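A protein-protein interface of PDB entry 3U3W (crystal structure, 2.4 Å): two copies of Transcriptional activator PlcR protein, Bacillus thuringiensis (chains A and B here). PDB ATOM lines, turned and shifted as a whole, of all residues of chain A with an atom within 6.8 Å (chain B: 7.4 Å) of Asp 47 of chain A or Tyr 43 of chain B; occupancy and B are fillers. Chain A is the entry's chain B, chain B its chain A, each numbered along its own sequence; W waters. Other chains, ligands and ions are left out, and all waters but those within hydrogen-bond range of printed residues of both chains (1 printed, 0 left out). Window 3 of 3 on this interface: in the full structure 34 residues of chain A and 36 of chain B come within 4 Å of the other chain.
Of the 10 printed residues of chain A, 4 touch a printed residue of chain B. Printed residues of chain A that touch a printed residue of chain B: Pro 44, Met 46, Asp 47 and Leu 49. Of the 18 printed residues of chain B, 5 touch a printed residue of chain A. Hydrophobic or aromatic side chains of chain B that line the printed part of chain A: Leu 6, Tyr 43, Pro 44, Met 46 and Tyr 64. Along chain B the printed residues that touch a printed residue of chain A span positions 6 to 64.
The side-chain hydroxyl (OG) of Ser 45 of chain A sits at hydrogen-bond distance from the side-chain carboxylate (OD1) of Asp 47 of chain A (2.8 Å).
Pro 44 of chain A touches Met 46 of chain B, and with the chains exchanged Met 46 of chain A touches Pro 44 of chain B. Positions printed for both chains: 44, 45, 46 and 48.
Water W1 lies within hydrogen-bond range of O of Pro 44 of chain B (2.8 Å) and N of Met 46 of chain A (3.0 Å).
Of the printed residues of chain B, Asp 47 of chain A touches Tyr 43. Of the printed residues of chain A, Pro 44 of chain B touches Met 46 (3.8 Å). Printed residues of chain B within 4 Å of Met 46 of chain A: Leu 6, Pro 44 and Tyr 64. Printed residues of chain A within 4 Å of Leu 6 of chain B: Met 46. Gln 50 of chain A touches none of the printed residues of chain B.
Among the printed residues, pairs that only touch across the chains: Met 46 of chain A with Leu 6 of chain B (3.5 Å), Met 46 of chain A with Tyr 64 of chain B (3.5 Å), Leu 49 of chain A with Tyr 64 of chain B (3.5 Å), Leu 49 of chain A with Met 46 of chain B (3.7 Å), Asp 47 of chain A with Tyr 43 of chain B (3.8 Å), Met 46 of chain A with Pro 44 of chain B (3.8 Å) and Pro 44 of chain A with Met 46 of chain B (3.8 Å).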
ATOM      1  N   ILE A  28       3.173 -12.332   1.767  1.00  0.00           N
ATOM      2  CA  ILE A  28       3.774 -13.270   0.833  1.00  0.00           C
ATOM      3  C   ILE A  28       2.726 -13.824  -0.122  1.00  0.00           C
ATOM      4  O   ILE A  28       2.891 -13.790  -1.346  1.00  0.00           O
ATOM      5  CB  ILE A  28       4.420 -14.440   1.584  1.00  0.00           C
ATOM      6  CG1 ILE A  28       5.501 -13.934   2.544  1.00  0.00           C
ATOM      7  CG2 ILE A  28       4.995 -15.453   0.600  1.00  0.00           C
ATOM      8  CD1 ILE A  28       6.189 -15.047   3.308  1.00  0.00           C
ATOM      9  N   PRO A  44       5.556 -24.135  -5.203  1.00  0.00           N
ATOM     10  CA  PRO A  44       5.469 -22.676  -5.059  1.00  0.00           C
ATOM     11  C   PRO A  44       6.417 -21.926  -5.989  1.00  0.00           C
ATOM     12  O   PRO A  44       7.482 -22.429  -6.326  1.00  0.00           O
ATOM     13  CB  PRO A  44       5.843 -22.447  -3.592  1.00  0.00           C
ATOM     14  CG  PRO A  44       6.733 -23.598  -3.251  1.00  0.00           C
ATOM     15  CD  PRO A  44       6.244 -24.771  -4.064  1.00  0.00           C
ATOM     16  N   SER A  45       6.013 -20.730  -6.405  1.00  0.00           N
ATOM     17  CA  SER A  45       6.847 -19.877  -7.257  1.00  0.00           C
ATOM     18  C   SER A  45       8.004 -19.219  -6.500  1.00  0.00           C
ATOM     19  O   SER A  45       7.986 -19.115  -5.269  1.00  0.00           O
ATOM     20  CB  SER A  45       5.992 -18.817  -7.963  1.00  0.00           C
ATOM     21  OG  SER A  45       4.899 -18.412  -7.154  1.00  0.00           O
ATOM     22  N   MET A  46       9.008 -18.775  -7.249  1.00  0.00           N
ATOM     23  CA  MET A  46      10.224 -18.218  -6.657  1.00  0.00           C
ATOM     24  C   MET A  46       9.919 -17.149  -5.612  1.00  0.00           C
ATOM     25  O   MET A  46      10.482 -17.153  -4.519  1.00  0.00           O
ATOM     26  CB  MET A  46      11.143 -17.657  -7.742  1.00  0.00           C
ATOM     27  CG  MET A  46      11.532 -18.688  -8.793  1.00  0.00           C
ATOM     28  SD  MET A  46      12.692 -18.039 -10.003  1.00  0.00           S
ATOM     29  CE  MET A  46      14.180 -17.885  -9.011  1.00  0.00           C
ATOM     30  N   ASP A  47       9.025 -16.227  -5.950  1.00  0.00           N
ATOM     31  CA  ASP A  47       8.644 -15.180  -5.013  1.00  0.00           C
ATOM     32  C   ASP A  47       8.122 -15.791  -3.710  1.00  0.00           C
ATOM     33  O   ASP A  47       8.618 -15.481  -2.625  1.00  0.00           O
ATOM     34  CB  ASP A  47       7.628 -14.210  -5.639  1.00  0.00           C
ATOM     35  CG  ASP A  47       6.542 -14.922  -6.437  1.00  0.00           C
ATOM     36  OD1 ASP A  47       6.328 -16.134  -6.216  1.00  0.00           O
ATOM     37  OD2 ASP A  47       5.894 -14.269  -7.285  1.00  0.00           O
ATOM     38  N   ILE A  48       7.142 -16.680  -3.819  1.00  0.00           N
ATOM     39  CA  ILE A  48       6.554 -17.295  -2.627  1.00  0.00           C
ATOM     40  C   ILE A  48       7.536 -18.185  -1.853  1.00  0.00           C
ATOM     41  O   ILE A  48       7.593 -18.120  -0.622  1.00  0.00           O
ATOM     42  CB  ILE A  48       5.243 -18.044  -2.948  1.00  0.00           C
ATOM     43  CG1 ILE A  48       4.225 -17.058  -3.541  1.00  0.00           C
ATOM     44  CG2 ILE A  48       4.680 -18.678  -1.699  1.00  0.00           C
ATOM     45  CD1 ILE A  48       2.837 -17.634  -3.796  1.00  0.00           C
ATOM     46  N   LEU A  49       8.319 -18.994  -2.564  1.00  0.00           N
ATOM     47  CA  LEU A  49       9.313 -19.832  -1.901  1.00  0.00           C
ATOM     48  C   LEU A  49      10.330 -18.975  -1.171  1.00  0.00           C
ATOM     49  O   LEU A  49      10.715 -19.274  -0.044  1.00  0.00           O
ATOM     50  CB  LEU A  49      10.045 -20.724  -2.904  1.00  0.00           C
ATOM     51  CG  LEU A  49      10.974 -21.706  -2.190  1.00  0.00           C
ATOM     52  CD1 LEU A  49      10.190 -22.626  -1.221  1.00  0.00           C
ATOM     53  CD2 LEU A  49      11.763 -22.521  -3.190  1.00  0.00           C
ATOM     54  N   GLN A  50      10.763 -17.915  -1.840  1.00  0.00           N
ATOM     55  CA  GLN A  50      11.771 -17.002  -1.313  1.00  0.00           C
ATOM     56  C   GLN A  50      11.310 -16.378  -0.003  1.00  0.00           C
ATOM     57  O   GLN A  50      12.021 -16.397   0.989  1.00  0.00           O
ATOM     58  CB  GLN A  50      12.057 -15.922  -2.350  1.00  0.00           C
ATOM     59  CG  GLN A  50      12.285 -14.542  -1.784  1.00  0.00           C
ATOM     60  CD  GLN A  50      13.686 -14.373  -1.280  1.00  0.00           C
ATOM     61  OE1 GLN A  50      14.645 -14.661  -1.996  1.00  0.00           O
ATOM     62  NE2 GLN A  50      13.824 -13.917  -0.038  1.00  0.00           N
ATOM     63  N   GLY A  51      10.101 -15.832  -0.016  1.00  0.00           N
ATOM     64  CA  GLY A  51       9.474 -15.294   1.176  1.00  0.00           C
ATOM     65  C   GLY A  51       9.347 -16.322   2.278  1.00  0.00           C
ATOM     66  O   GLY A  51       9.748 -16.074   3.416  1.00  0.00           O
ATOM     67  N   ILE A  52       8.796 -17.487   1.949  1.00  0.00           N
ATOM     68  CA  ILE A  52       8.689 -18.557   2.938  1.00  0.00           C
ATOM     69  C   ILE A  52      10.046 -18.970   3.531  1.00  0.00           C
ATOM     70  O   ILE A  52      10.164 -19.148   4.738  1.00  0.00           O
ATOM     71  CB  ILE A  52       7.962 -19.785   2.386  1.00  0.00           C
ATOM     72  CG1 ILE A  52       6.508 -19.432   2.067  1.00  0.00           C
ATOM     73  CG2 ILE A  52       8.030 -20.928   3.396  1.00  0.00           C
ATOM     74  CD1 ILE A  52       5.761 -20.553   1.406  1.00  0.00           C
ATOM     75  N   ALA B   3      10.097  -9.830 -13.863  1.00  0.00           N
ATOM     76  CA  ALA B   3      11.518  -9.830 -13.520  1.00  0.00           C
ATOM     77  C   ALA B   3      12.405 -10.272 -14.688  1.00  0.00           C
ATOM     78  O   ALA B   3      12.581 -11.469 -14.932  1.00  0.00           O
ATOM     79  CB  ALA B   3      11.773 -10.708 -12.300  1.00  0.00           C
ATOM     80  N   GLU B   4      12.973  -9.307 -15.406  1.00  0.00           N
ATOM     81  CA  GLU B   4      13.817  -9.630 -16.549  1.00  0.00           C
ATOM     82  C   GLU B   4      15.286  -9.838 -16.164  1.00  0.00           C
ATOM     83  O   GLU B   4      16.095 -10.273 -16.990  1.00  0.00           O
ATOM     84  CB  GLU B   4      13.700  -8.567 -17.645  1.00  0.00           C
ATOM     85  CG  GLU B   4      13.957  -9.129 -19.044  1.00  0.00           C
ATOM     86  CD  GLU B   4      14.727  -8.177 -19.937  1.00  0.00           C
ATOM     87  OE1 GLU B   4      14.977  -7.030 -19.509  1.00  0.00           O
ATOM     88  OE2 GLU B   4      15.086  -8.582 -21.064  1.00  0.00           O
ATOM     89  N   LEU B   6      16.531 -12.022 -13.812  1.00  0.00           N
ATOM     90  CA  LEU B   6      16.753 -13.473 -13.819  1.00  0.00           C
ATOM     91  C   LEU B   6      16.974 -13.977 -15.240  1.00  0.00           C
ATOM     92  O   LEU B   6      17.946 -14.680 -15.512  1.00  0.00           O
ATOM     93  CB  LEU B   6      15.574 -14.226 -13.190  1.00  0.00           C
ATOM     94  CG  LEU B   6      15.649 -15.760 -13.236  1.00  0.00           C
ATOM     95  CD1 LEU B   6      16.943 -16.263 -12.629  1.00  0.00           C
ATOM     96  CD2 LEU B   6      14.460 -16.402 -12.532  1.00  0.00           C
ATOM     97  N   GLY B   7      16.065 -13.594 -16.137  1.00  0.00           N
ATOM     98  CA  GLY B   7      16.118 -14.002 -17.529  1.00  0.00           C
ATOM     99  C   GLY B   7      17.463 -13.830 -18.210  1.00  0.00           C
ATOM    100  O   GLY B   7      17.996 -14.783 -18.782  1.00  0.00           O
ATOM    101  N   GLU B  33      10.111 -22.480 -23.778  1.00  0.00           N
ATOM    102  CA  GLU B  33       9.994 -22.067 -22.380  1.00  0.00           C
ATOM    103  C   GLU B  33      11.302 -21.462 -21.872  1.00  0.00           C
ATOM    104  O   GLU B  33      11.285 -20.530 -21.076  1.00  0.00           O
ATOM    105  CB  GLU B  33       9.579 -23.244 -21.494  1.00  0.00           C
ATOM    106  CG  GLU B  33       9.441 -22.923 -20.015  1.00  0.00           C
ATOM    107  CD  GLU B  33       8.263 -22.010 -19.707  1.00  0.00           C
ATOM    108  OE1 GLU B  33       7.609 -21.530 -20.659  1.00  0.00           O
ATOM    109  OE2 GLU B  33       7.996 -21.772 -18.504  1.00  0.00           O
ATOM    110  N   ARG B  36      11.153 -18.026 -23.177  1.00  0.00           N
ATOM    111  CA  ARG B  36      10.274 -17.181 -22.389  1.00  0.00           C
ATOM    112  C   ARG B  36      10.862 -16.865 -21.014  1.00  0.00           C
ATOM    113  O   ARG B  36      10.633 -15.785 -20.475  1.00  0.00           O
ATOM    114  CB  ARG B  36       8.882 -17.801 -22.263  1.00  0.00           C
ATOM    115  CG  ARG B  36       8.051 -17.771 -23.542  1.00  0.00           C
ATOM    116  CD  ARG B  36       6.590 -18.020 -23.210  1.00  0.00           C
ATOM    117  NE  ARG B  36       5.839 -18.616 -24.310  1.00  0.00           N
ATOM    118  CZ  ARG B  36       5.138 -17.920 -25.196  1.00  0.00           C
ATOM    119  NH1 ARG B  36       5.099 -16.595 -25.123  1.00  0.00           N
ATOM    120  NH2 ARG B  36       4.477 -18.549 -26.154  1.00  0.00           N
ATOM    121  N   ILE B  37      11.616 -17.807 -20.453  1.00  0.00           N
ATOM    122  CA  ILE B  37      12.346 -17.575 -19.208  1.00  0.00           C
ATOM    123  C   ILE B  37      13.437 -16.504 -19.370  1.00  0.00           C
ATOM    124  O   ILE B  37      13.592 -15.636 -18.506  1.00  0.00           O
ATOM    125  CB  ILE B  37      12.959 -18.879 -18.653  1.00  0.00           C
ATOM    126  CG1 ILE B  37      11.854 -19.800 -18.145  1.00  0.00           C
ATOM    127  CG2 ILE B  37      13.940 -18.591 -17.522  1.00  0.00           C
ATOM    128  CD1 ILE B  37      12.334 -21.182 -17.838  1.00  0.00           C
ATOM    129  N   GLY B  40      12.094 -12.806 -19.631  1.00  0.00           N
ATOM    130  CA  GLY B  40      11.514 -12.255 -18.423  1.00  0.00           C
ATOM    131  C   GLY B  40      10.007 -12.412 -18.329  1.00  0.00           C
ATOM    132  O   GLY B  40       9.391 -11.946 -17.376  1.00  0.00           O
ATOM    133  N   ALA B  41       9.414 -13.080 -19.312  1.00  0.00           N
ATOM    134  CA  ALA B  41       7.958 -13.199 -19.413  1.00  0.00           C
ATOM    135  C   ALA B  41       7.390 -14.202 -18.422  1.00  0.00           C
ATOM    136  O   ALA B  41       6.177 -14.318 -18.256  1.00  0.00           O
ATOM    137  CB  ALA B  41       7.564 -13.600 -20.831  1.00  0.00           C
ATOM    138  N   VAL B  42       8.274 -14.922 -17.754  1.00  0.00           N
ATOM    139  CA  VAL B  42       7.851 -16.035 -16.945  1.00  0.00           C
ATOM    140  C   VAL B  42       8.840 -16.301 -15.817  1.00  0.00           C
ATOM    141  O   VAL B  42      10.046 -16.167 -15.995  1.00  0.00           O
ATOM    142  CB  VAL B  42       7.691 -17.290 -17.835  1.00  0.00           C
ATOM    143  CG1 VAL B  42       8.201 -18.520 -17.130  1.00  0.00           C
ATOM    144  CG2 VAL B  42       6.240 -17.456 -18.266  1.00  0.00           C
ATOM    145  N   TYR B  43       8.314 -16.645 -14.650  1.00  0.00           N
ATOM    146  CA  TYR B  43       9.112 -17.253 -13.599  1.00  0.00           C
ATOM    147  C   TYR B  43       9.062 -18.765 -13.801  1.00  0.00           C
ATOM    148  O   TYR B  43       7.988 -19.326 -14.021  1.00  0.00           O
ATOM    149  CB  TYR B  43       8.537 -16.927 -12.220  1.00  0.00           C
ATOM    150  CG  TYR B  43       8.897 -15.568 -11.659  1.00  0.00           C
ATOM    151  CD1 TYR B  43       9.819 -14.738 -12.293  1.00  0.00           C
ATOM    152  CD2 TYR B  43       8.324 -15.125 -10.473  1.00  0.00           C
ATOM    153  CE1 TYR B  43      10.141 -13.498 -11.764  1.00  0.00           C
ATOM    154  CE2 TYR B  43       8.640 -13.897  -9.938  1.00  0.00           C
ATOM    155  CZ  TYR B  43       9.545 -13.082 -10.582  1.00  0.00           C
ATOM    156  OH  TYR B  43       9.843 -11.852 -10.025  1.00  0.00           O
ATOM    157  N   PRO B  44      10.219 -19.433 -13.722  1.00  0.00           N
ATOM    158  CA  PRO B  44      10.229 -20.889 -13.874  1.00  0.00           C
ATOM    159  C   PRO B  44       9.888 -21.600 -12.565  1.00  0.00           C
ATOM    160  O   PRO B  44      10.158 -21.073 -11.492  1.00  0.00           O
ATOM    161  CB  PRO B  44      11.678 -21.180 -14.277  1.00  0.00           C
ATOM    162  CG  PRO B  44      12.465 -20.115 -13.566  1.00  0.00           C
ATOM    163  CD  PRO B  44      11.578 -18.878 -13.581  1.00  0.00           C
ATOM    164  N   SER B  45       9.291 -22.785 -12.667  1.00  0.00           N
ATOM    165  CA  SER B  45       9.015 -23.626 -11.499  1.00  0.00           C
ATOM    166  C   SER B  45      10.286 -24.259 -10.930  1.00  0.00           C
ATOM    167  O   SER B  45      11.349 -24.215 -11.553  1.00  0.00           O
ATOM    168  CB  SER B  45       8.001 -24.722 -11.845  1.00  0.00           C
ATOM    169  OG  SER B  45       7.616 -24.658 -13.210  1.00  0.00           O
ATOM    170  N   MET B  46      10.165 -24.856  -9.749  1.00  0.00           N
ATOM    171  CA  MET B  46      11.321 -25.428  -9.067  1.00  0.00           C
ATOM    172  C   MET B  46      12.033 -26.495  -9.906  1.00  0.00           C
ATOM    173  O   MET B  46      13.254 -26.471 -10.049  1.00  0.00           O
ATOM    174  CB  MET B  46      10.923 -25.968  -7.696  1.00  0.00           C
ATOM    175  CG  MET B  46      10.421 -24.879  -6.746  1.00  0.00           C
ATOM    176  SD  MET B  46       9.904 -25.545  -5.157  1.00  0.00           S
ATOM    177  CE  MET B  46      11.485 -25.962  -4.421  1.00  0.00           C
ATOM    178  N   ILE B  48      12.092 -26.997 -13.258  1.00  0.00           N
ATOM    179  CA  ILE B  48      12.820 -26.354 -14.351  1.00  0.00           C
ATOM    180  C   ILE B  48      14.042 -25.527 -13.911  1.00  0.00           C
ATOM    181  O   ILE B  48      15.090 -25.577 -14.561  1.00  0.00           O
ATOM    182  CB  ILE B  48      11.872 -25.522 -15.236  1.00  0.00           C
ATOM    183  CG1 ILE B  48      10.777 -26.436 -15.805  1.00  0.00           C
ATOM    184  CG2 ILE B  48      12.642 -24.827 -16.351  1.00  0.00           C
ATOM    185  CD1 ILE B  48       9.809 -25.769 -16.759  1.00  0.00           C
ATOM    186  N   TYR B  64      18.104 -16.740  -7.187  1.00  0.00           N
ATOM    187  CA  TYR B  64      17.295 -15.989  -6.250  1.00  0.00           C
ATOM    188  C   TYR B  64      17.931 -14.638  -5.916  1.00  0.00           C
ATOM    189  O   TYR B  64      17.236 -13.625  -5.864  1.00  0.00           O
ATOM    190  CB  TYR B  64      17.010 -16.814  -5.003  1.00  0.00           C
ATOM    191  CG  TYR B  64      15.956 -17.865  -5.250  1.00  0.00           C
ATOM    192  CD1 TYR B  64      14.611 -17.594  -5.016  1.00  0.00           C
ATOM    193  CD2 TYR B  64      16.299 -19.117  -5.744  1.00  0.00           C
ATOM    194  CE1 TYR B  64      13.636 -18.549  -5.253  1.00  0.00           C
ATOM    195  CE2 TYR B  64      15.330 -20.078  -5.980  1.00  0.00           C
ATOM    196  CZ  TYR B  64      14.003 -19.786  -5.733  1.00  0.00           C
ATOM    197  OH  TYR B  64      13.045 -20.737  -5.967  1.00  0.00           O
ATOM    198  N   LEU B  67      17.285 -12.054  -8.404  1.00  0.00           N
ATOM    199  CA  LEU B  67      15.860 -11.980  -8.718  1.00  0.00           C
ATOM    200  C   LEU B  67      15.259 -10.571  -8.647  1.00  0.00           C
ATOM    201  O   LEU B  67      14.479 -10.186  -9.515  1.00  0.00           O
ATOM    202  CB  LEU B  67      15.063 -12.948  -7.833  1.00  0.00           C
ATOM    203  CG  LEU B  67      13.601 -13.186  -8.211  1.00  0.00           C
ATOM    204  CD1 LEU B  67      13.504 -13.916  -9.539  1.00  0.00           C
ATOM    205  CD2 LEU B  67      12.895 -13.960  -7.112  1.00  0.00           C
ATOM    206  N   ILE B  68      15.612  -9.801  -7.622  1.00  0.00           N
ATOM    207  CA  ILE B  68      14.917  -8.531  -7.370  1.00  0.00           C
ATOM    208  C   ILE B  68      15.793  -7.274  -7.472  1.00  0.00           C
ATOM    209  O   ILE B  68      15.438  -6.318  -8.174  1.00  0.00           O
ATOM    210  CB  ILE B  68      14.177  -8.541  -6.003  1.00  0.00           C
ATOM    211  CG1 ILE B  68      13.183  -9.711  -5.929  1.00  0.00           C
ATOM    212  CG2 ILE B  68      13.488  -7.194  -5.750  1.00  0.00           C
ATOM    213  CD1 ILE B  68      12.374  -9.761  -4.638  1.00  0.00           C
HETATM  214  O   HOH W   1       8.591 -19.207 -10.164  1.00  0.00           O
